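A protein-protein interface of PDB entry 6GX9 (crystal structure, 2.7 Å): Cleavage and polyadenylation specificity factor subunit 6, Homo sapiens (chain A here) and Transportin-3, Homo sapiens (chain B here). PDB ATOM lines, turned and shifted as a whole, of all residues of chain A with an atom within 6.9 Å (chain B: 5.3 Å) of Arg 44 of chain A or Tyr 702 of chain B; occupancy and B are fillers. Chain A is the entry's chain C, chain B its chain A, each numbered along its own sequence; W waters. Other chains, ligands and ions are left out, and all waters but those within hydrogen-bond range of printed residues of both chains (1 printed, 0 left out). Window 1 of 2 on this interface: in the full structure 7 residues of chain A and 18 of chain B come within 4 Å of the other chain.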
ATOM      1  N   TYR A  41       4.754  11.541 -12.221  1.00  0.00           N
ATOM      2  CA  TYR A  41       3.995  10.892 -13.282  1.00  0.00           C
ATOM      3  C   TYR A  41       3.513  11.866 -14.349  1.00  0.00           C
ATOM      4  O   TYR A  41       2.999  11.422 -15.382  1.00  0.00           O
ATOM      5  CB  TYR A  41       2.797  10.142 -12.691  1.00  0.00           C
ATOM      6  CG  TYR A  41       1.910  10.984 -11.798  1.00  0.00           C
ATOM      7  CD1 TYR A  41       0.862  11.727 -12.328  1.00  0.00           C
ATOM      8  CD2 TYR A  41       2.114  11.029 -10.424  1.00  0.00           C
ATOM      9  CE1 TYR A  41       0.045  12.497 -11.515  1.00  0.00           C
ATOM     10  CE2 TYR A  41       1.303  11.795  -9.603  1.00  0.00           C
ATOM     11  CZ  TYR A  41       0.271  12.525 -10.154  1.00  0.00           C
ATOM     12  OH  TYR A  41      -0.538  13.288  -9.341  1.00  0.00           O
ATOM     13  N   ARG A  42       3.655  13.170 -14.124  1.00  0.00           N
ATOM     14  CA  ARG A  42       3.242  14.180 -15.090  1.00  0.00           C
ATOM     15  C   ARG A  42       4.400  14.473 -16.035  1.00  0.00           C
ATOM     16  O   ARG A  42       5.474  14.899 -15.594  1.00  0.00           O
ATOM     17  CB  ARG A  42       2.798  15.457 -14.377  1.00  0.00           C
ATOM     18  CG  ARG A  42       2.243  16.522 -15.309  1.00  0.00           C
ATOM     19  CD  ARG A  42       2.296  17.900 -14.670  1.00  0.00           C
ATOM     20  NE  ARG A  42       1.752  18.929 -15.552  1.00  0.00           N
ATOM     21  CZ  ARG A  42       1.962  20.231 -15.398  1.00  0.00           C
ATOM     22  NH1 ARG A  42       2.716  20.669 -14.398  1.00  0.00           N
ATOM     23  NH2 ARG A  42       1.427  21.096 -16.248  1.00  0.00           N
ATOM     24  N   GLU A  43       4.184  14.254 -17.330  1.00  0.00           N
ATOM     25  CA  GLU A  43       5.205  14.491 -18.340  1.00  0.00           C
ATOM     26  C   GLU A  43       4.644  15.392 -19.430  1.00  0.00           C
ATOM     27  O   GLU A  43       3.576  15.115 -19.984  1.00  0.00           O
ATOM     28  CB  GLU A  43       5.709  13.175 -18.943  1.00  0.00           C
ATOM     29  CG  GLU A  43       6.894  13.352 -19.882  1.00  0.00           C
ATOM     30  CD  GLU A  43       7.149  12.130 -20.737  1.00  0.00           C
ATOM     31  OE1 GLU A  43       7.098  11.007 -20.194  1.00  0.00           O
ATOM     32  OE2 GLU A  43       7.403  12.292 -21.950  1.00  0.00           O
ATOM     33  N   ARG A  44       5.364  16.470 -19.729  1.00  0.00           N
ATOM     34  CA  ARG A  44       4.991  17.387 -20.801  1.00  0.00           C
ATOM     35  C   ARG A  44       6.065  17.425 -21.886  1.00  0.00           C
ATOM     36  O   ARG A  44       7.183  16.954 -21.680  1.00  0.00           O
ATOM     37  CB  ARG A  44       4.762  18.796 -20.247  1.00  0.00           C
ATOM     38  CG  ARG A  44       3.609  18.908 -19.266  1.00  0.00           C
ATOM     39  CD  ARG A  44       2.279  18.722 -19.973  1.00  0.00           C
ATOM     40  NE  ARG A  44       1.151  18.728 -19.046  1.00  0.00           N
ATOM     41  CZ  ARG A  44       0.649  17.637 -18.480  1.00  0.00           C
ATOM     42  NH1 ARG A  44       1.177  16.449 -18.747  1.00  0.00           N
ATOM     43  NH2 ARG A  44      -0.382  17.730 -17.650  1.00  0.00           N
ATOM     44  N   SEP A  45       5.723  17.986 -23.042  1.00  0.00           N
ATOM     45  CA  SEP A  45       6.693  18.161 -24.119  1.00  0.00           C
ATOM     46  CB  SEP A  45       5.988  18.243 -25.477  1.00  0.00           C
ATOM     47  OG  SEP A  45       5.059  19.316 -25.520  1.00  0.00           O
ATOM     48  C   SEP A  45       7.534  19.411 -23.871  1.00  0.00           C
ATOM     49  O   SEP A  45       7.076  20.362 -23.237  1.00  0.00           O
ATOM     50  P   SEP A  45       4.200  19.254 -26.883  1.00  0.00           P
ATOM     51  O1P SEP A  45       5.182  19.425 -28.147  1.00  0.00           O
ATOM     52  O2P SEP A  45       3.096  20.425 -26.883  1.00  0.00           O
ATOM     53  O3P SEP A  45       3.467  17.826 -26.984  1.00  0.00           O
ATOM     54  N   ARG A  46       8.768  19.405 -24.366  1.00  0.00           N
ATOM     55  CA  ARG A  46       9.685  20.522 -24.147  1.00  0.00           C
ATOM     56  C   ARG A  46       9.389  21.684 -25.093  1.00  0.00           C
ATOM     57  O   ARG A  46       8.458  21.621 -25.898  1.00  0.00           O
ATOM     58  CB  ARG A  46      11.134  20.065 -24.316  1.00  0.00           C
ATOM     59  N   GLU B 660      -3.615  10.821 -15.911  1.00  0.00           N
ATOM     60  CA  GLU B 660      -2.416  11.402 -16.506  1.00  0.00           C
ATOM     61  C   GLU B 660      -1.738  10.422 -17.454  1.00  0.00           C
ATOM     62  O   GLU B 660      -1.295  10.806 -18.543  1.00  0.00           O
ATOM     63  CB  GLU B 660      -1.450  11.842 -15.406  1.00  0.00           C
ATOM     64  CG  GLU B 660      -0.286  12.685 -15.895  1.00  0.00           C
ATOM     65  CD  GLU B 660      -0.708  14.085 -16.296  1.00  0.00           C
ATOM     66  OE1 GLU B 660      -1.427  14.742 -15.513  1.00  0.00           O
ATOM     67  OE2 GLU B 660      -0.324  14.525 -17.399  1.00  0.00           O
ATOM     68  N   ARG B 667      -1.769  10.886 -26.078  1.00  0.00           N
ATOM     69  CA  ARG B 667      -0.905  11.878 -26.707  1.00  0.00           C
ATOM     70  C   ARG B 667      -0.066  11.249 -27.813  1.00  0.00           C
ATOM     71  O   ARG B 667      -0.131  11.665 -28.976  1.00  0.00           O
ATOM     72  CB  ARG B 667      -0.010  12.531 -25.651  1.00  0.00           C
ATOM     73  CG  ARG B 667       1.225  13.218 -26.211  1.00  0.00           C
ATOM     74  CD  ARG B 667       1.755  14.262 -25.245  1.00  0.00           C
ATOM     75  NE  ARG B 667       2.779  13.762 -24.332  1.00  0.00           N
ATOM     76  CZ  ARG B 667       4.087  13.923 -24.519  1.00  0.00           C
ATOM     77  NH1 ARG B 667       4.534  14.566 -25.588  1.00  0.00           N
ATOM     78  NH2 ARG B 667       4.949  13.446 -23.632  1.00  0.00           N
ATOM     79  N   SER B 698      -5.784  18.859 -15.114  1.00  0.00           N
ATOM     80  CA  SER B 698      -5.214  19.792 -16.081  1.00  0.00           C
ATOM     81  C   SER B 698      -4.671  19.093 -17.320  1.00  0.00           C
ATOM     82  O   SER B 698      -4.474  19.752 -18.347  1.00  0.00           O
ATOM     83  CB  SER B 698      -4.110  20.628 -15.430  1.00  0.00           C
ATOM     84  OG  SER B 698      -2.972  19.839 -15.136  1.00  0.00           O
ATOM     85  N   CYS B 699      -4.428  17.781 -17.255  1.00  0.00           N
ATOM     86  CA  CYS B 699      -3.906  17.063 -18.412  1.00  0.00           C
ATOM     87  C   CYS B 699      -4.908  16.970 -19.556  1.00  0.00           C
ATOM     88  O   CYS B 699      -4.515  16.607 -20.670  1.00  0.00           O
ATOM     89  CB  CYS B 699      -3.449  15.659 -18.007  1.00  0.00           C
ATOM     90  SG  CYS B 699      -4.718  14.626 -17.242  1.00  0.00           S
ATOM     91  N   PHE B 700      -6.184  17.281 -19.315  1.00  0.00           N
ATOM     92  CA  PHE B 700      -7.126  17.391 -20.424  1.00  0.00           C
ATOM     93  C   PHE B 700      -6.889  18.663 -21.225  1.00  0.00           C
ATOM     94  O   PHE B 700      -7.071  18.668 -22.447  1.00  0.00           O
ATOM     95  CB  PHE B 700      -8.565  17.347 -19.909  1.00  0.00           C
ATOM     96  CG  PHE B 700      -8.990  15.993 -19.420  1.00  0.00           C
ATOM     97  CD1 PHE B 700      -9.241  14.968 -20.315  1.00  0.00           C
ATOM     98  CD2 PHE B 700      -9.144  15.748 -18.065  1.00  0.00           C
ATOM     99  CE1 PHE B 700      -9.633  13.719 -19.868  1.00  0.00           C
ATOM    100  CE2 PHE B 700      -9.537  14.502 -17.611  1.00  0.00           C
ATOM    101  CZ  PHE B 700      -9.782  13.487 -18.516  1.00  0.00           C
ATOM    102  N   LEU B 701      -6.487  19.748 -20.557  1.00  0.00           N
ATOM    103  CA  LEU B 701      -6.108  20.960 -21.275  1.00  0.00           C
ATOM    104  C   LEU B 701      -4.866  20.724 -22.124  1.00  0.00           C
ATOM    105  O   LEU B 701      -4.752  21.264 -23.232  1.00  0.00           O
ATOM    106  CB  LEU B 701      -5.873  22.104 -20.289  1.00  0.00           C
ATOM    107  CG  LEU B 701      -7.039  22.478 -19.374  1.00  0.00           C
ATOM    108  CD1 LEU B 701      -6.617  23.556 -18.384  1.00  0.00           C
ATOM    109  CD2 LEU B 701      -8.234  22.933 -20.196  1.00  0.00           C
ATOM    110  N   TYR B 702      -3.929  19.915 -21.625  1.00  0.00           N
ATOM    111  CA  TYR B 702      -2.743  19.599 -22.411  1.00  0.00           C
ATOM    112  C   TYR B 702      -3.088  18.687 -23.580  1.00  0.00           C
ATOM    113  O   TYR B 702      -2.606  18.897 -24.699  1.00  0.00           O
ATOM    114  CB  TYR B 702      -1.678  18.957 -21.524  1.00  0.00           C
ATOM    115  CG  TYR B 702      -0.451  18.507 -22.283  1.00  0.00           C
ATOM    116  CD1 TYR B 702       0.294  19.410 -23.029  1.00  0.00           C
ATOM    117  CD2 TYR B 702      -0.031  17.184 -22.244  1.00  0.00           C
ATOM    118  CE1 TYR B 702       1.417  19.010 -23.723  1.00  0.00           C
ATOM    119  CE2 TYR B 702       1.096  16.773 -22.934  1.00  0.00           C
ATOM    120  CZ  TYR B 702       1.815  17.691 -23.672  1.00  0.00           C
ATOM    121  OH  TYR B 702       2.936  17.296 -24.363  1.00  0.00           O
ATOM    122  N   LEU B 703      -3.917  17.669 -23.340  1.00  0.00           N
ATOM    123  CA  LEU B 703      -4.333  16.790 -24.426  1.00  0.00           C
ATOM    124  C   LEU B 703      -5.093  17.564 -25.495  1.00  0.00           C
ATOM    125  O   LEU B 703      -4.960  17.281 -26.692  1.00  0.00           O
ATOM    126  CB  LEU B 703      -5.185  15.645 -23.878  1.00  0.00           C
ATOM    127  CG  LEU B 703      -5.668  14.609 -24.893  1.00  0.00           C
ATOM    128  CD1 LEU B 703      -4.497  14.062 -25.695  1.00  0.00           C
ATOM    129  CD2 LEU B 703      -6.411  13.485 -24.190  1.00  0.00           C
ATOM    130  N   GLY B 704      -5.886  18.555 -25.082  1.00  0.00           N
ATOM    131  CA  GLY B 704      -6.543  19.410 -26.054  1.00  0.00           C
ATOM    132  C   GLY B 704      -5.556  20.199 -26.891  1.00  0.00           C
ATOM    133  O   GLY B 704      -5.783  20.430 -28.081  1.00  0.00           O
ATOM    134  N   SER B 705      -4.439  20.614 -26.284  1.00  0.00           N
ATOM    135  CA  SER B 705      -3.417  21.335 -27.035  1.00  0.00           C
ATOM    136  C   SER B 705      -2.794  20.452 -28.106  1.00  0.00           C
ATOM    137  O   SER B 705      -2.446  20.935 -29.191  1.00  0.00           O
ATOM    138  CB  SER B 705      -2.339  21.873 -26.090  1.00  0.00           C
ATOM    139  OG  SER B 705      -1.571  20.827 -25.523  1.00  0.00           O
ATOM    140  N   ILE B 706      -2.642  19.154 -27.824  1.00  0.00           N
ATOM    141  CA  ILE B 706      -2.122  18.239 -28.835  1.00  0.00           C
ATOM    142  C   ILE B 706      -3.097  18.124 -29.997  1.00  0.00           C
ATOM    143  O   ILE B 706      -2.692  18.127 -31.166  1.00  0.00           O
ATOM    144  CB  ILE B 706      -1.812  16.865 -28.215  1.00  0.00           C
ATOM    145  CG1 ILE B 706      -0.609  16.964 -27.279  1.00  0.00           C
ATOM    146  CG2 ILE B 706      -1.549  15.832 -29.300  1.00  0.00           C
ATOM    147  CD1 ILE B 706      -0.905  16.512 -25.875  1.00  0.00           C
ATOM    148  N   ASP B 750      -0.634  26.310 -16.276  1.00  0.00           N
ATOM    149  CA  ASP B 750       0.357  25.851 -17.244  1.00  0.00           C
ATOM    150  C   ASP B 750      -0.314  25.251 -18.475  1.00  0.00           C
ATOM    151  O   ASP B 750      -0.074  25.687 -19.607  1.00  0.00           O
ATOM    152  CB  ASP B 750       1.289  24.834 -16.580  1.00  0.00           C
ATOM    153  CG  ASP B 750       2.361  24.307 -17.521  1.00  0.00           C
ATOM    154  OD1 ASP B 750       2.565  24.893 -18.606  1.00  0.00           O
ATOM    155  OD2 ASP B 750       3.003  23.296 -17.167  1.00  0.00           O
ATOM    156  N   ASP B 751      -1.153  24.234 -18.273  1.00  0.00           N
ATOM    157  CA  ASP B 751      -1.760  23.533 -19.397  1.00  0.00           C
ATOM    158  C   ASP B 751      -2.805  24.374 -20.123  1.00  0.00           C
ATOM    159  O   ASP B 751      -3.056  24.132 -21.309  1.00  0.00           O
ATOM    160  CB  ASP B 751      -2.376  22.220 -18.911  1.00  0.00           C
ATOM    161  CG  ASP B 751      -1.330  21.234 -18.425  1.00  0.00           C
ATOM    162  OD1 ASP B 751      -0.261  21.141 -19.066  1.00  0.00           O
ATOM    163  OD2 ASP B 751      -1.567  20.558 -17.400  1.00  0.00           O
ATOM    164  N   ARG B 754      -0.764  26.440 -22.490  1.00  0.00           N
ATOM    165  CA  ARG B 754      -0.276  25.526 -23.514  1.00  0.00           C
ATOM    166  C   ARG B 754      -1.336  25.331 -24.590  1.00  0.00           C
ATOM    167  O   ARG B 754      -1.030  25.355 -25.788  1.00  0.00           O
ATOM    168  CB  ARG B 754       0.101  24.184 -22.889  1.00  0.00           C
ATOM    169  CG  ARG B 754       1.521  24.087 -22.364  1.00  0.00           C
ATOM    170  CD  ARG B 754       1.707  22.799 -21.566  1.00  0.00           C
ATOM    171  NE  ARG B 754       3.074  22.633 -21.080  1.00  0.00           N
ATOM    172  CZ  ARG B 754       4.060  22.101 -21.797  1.00  0.00           C
ATOM    173  NH1 ARG B 754       5.273  21.989 -21.275  1.00  0.00           N
ATOM    174  NH2 ARG B 754       3.834  21.678 -23.036  1.00  0.00           N
HETATM  175  O   HOH W   1       3.450  15.340 -28.099  1.00  0.00           O
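The side-chain sulfur (SG) of Cys 699 of chain B sits close to the side-chain carboxylate (OE1) of Glu 660 of chain B, at 3.7 Å.
OH of Tyr 702 of chain B sits close to NH1 of Arg 667 of chain B (3.4 Å).
OG of Ser 698 of chain B sits at hydrogen-bond distance from OD2 of Asp 751 of chain B (2.8 Å).
NE of Arg 754 of chain B is in salt-bridge range of OD1 of Asp 750 of chain B (3.4 Å).
The guanidinium group (NH1) of Arg 44 of chain A lies within salt-bridge range of the side-chain carboxylate (OE2) of Glu 660 of chain B.
The side-chain carboxylate (OE2) of Glu 43 of chain A lies within salt-bridge range of the guanidinium group (NH2) of Arg 667 of chain B (3.2 Å).
The guanidinium group (NH1) of Arg 667 of chain B sits close to O3P of SEP 45 of chain A.
OH of Tyr 702 of chain B is in hydrogen-bond range of O3P of SEP 45 of chain A (2.7 Å).
The guanidinium group of Arg 42 of chain A is in salt-bridge range of the side-chain carboxylate of Asp 750 of chain B (2.9 Å).
The side-chain carboxylate (OD2) of Asp 751 of chain B is in salt-bridge range of the guanidinium group (NH2) of Arg 42 of chain A.
The side-chain carboxylate of Asp 751 of chain B lies within salt-bridge range of the guanidinium group of Arg 44 of chain A.
The guanidinium group (NH1) of Arg 754 of chain B is in hydrogen-bond range of O of SEP 45 of chain A.
Printed residues of chain B within 4 Å of Glu 43 of chain A: Arg 667.
Arg 44 of chain A touches just these residues of chain B: Glu 660 (2.8 Å), Cys 699 (3.7 Å), Tyr 702 (3.6 Å), Asp 751 (2.8 Å) and Arg 754 (3.4 Å).
Of the printed residues of chain A, Arg 667 of chain B touches Glu 43 (3.2 Å) and SEP 45 (3.7 Å).
Tyr 702 of chain B touches just these residues of chain A: Arg 44 (3.6 Å) and SEP 45 (2.7 Å).
Leu 703 of chain B touches none of the printed residues of chain A.
Of the printed residues of chain A, Arg 754 of chain B touches Arg 44 and SEP 45.
The nearest residue of chain A that does not touch Tyr 702 of chain B is Glu 43 of chain A (4.2 Å).
The nearest printed residue of chain A that does not touch Cys 699 of chain B is Arg 42 of chain A (6.4 Å).
Water W1 lies within hydrogen-bond range of O3P of SEP 45 of chain A (2.7 Å) and NH1 of Arg 667 of chain B (2.8 Å).
Glu 660 of chain B touches Tyr 41 of chain A (CG to O, 3.6 Å).
Arg 42 of chain A touches Glu 660 of chain B (CG to OE2, 3.9 Å).
Arg 44 of chain A touches Cys 699 of chain B (NH2 to CA, 3.7 Å).
Arg 44 of chain A touches Tyr 702 of chain B (CD to CG, 3.6 Å).
NH1 of Arg 754 of chain B touches CB of Arg 44 of chain A (3.4 Å).
Of the 6 printed residues of chain A, 5 touch a printed residue of chain B.
Hydrophobic or aromatic side chains of chain A within 4 Å of the printed part of chain B: Tyr 41.
Hydrophobic or aromatic side chains of chain B that line the printed part of chain A: Tyr 702.
Along chain B the printed residues that touch a printed residue of chain A span positions 660 to 754.
Among the printed residues, 13 pairs touch across the chains.
Among the printed residues, Asp or Glu carboxylates within 4 Å of a Lys or Arg side-chain nitrogen of the other chain: Arg 42 of chain A with Asp 750 of chain B, Arg 42 of chain A with Asp 751 of chain B, Glu 43 of chain A with Arg 667 of chain B, Arg 44 of chain A with Glu 660 of chain B and Arg 44 of chain A with Asp 751 of chain B.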
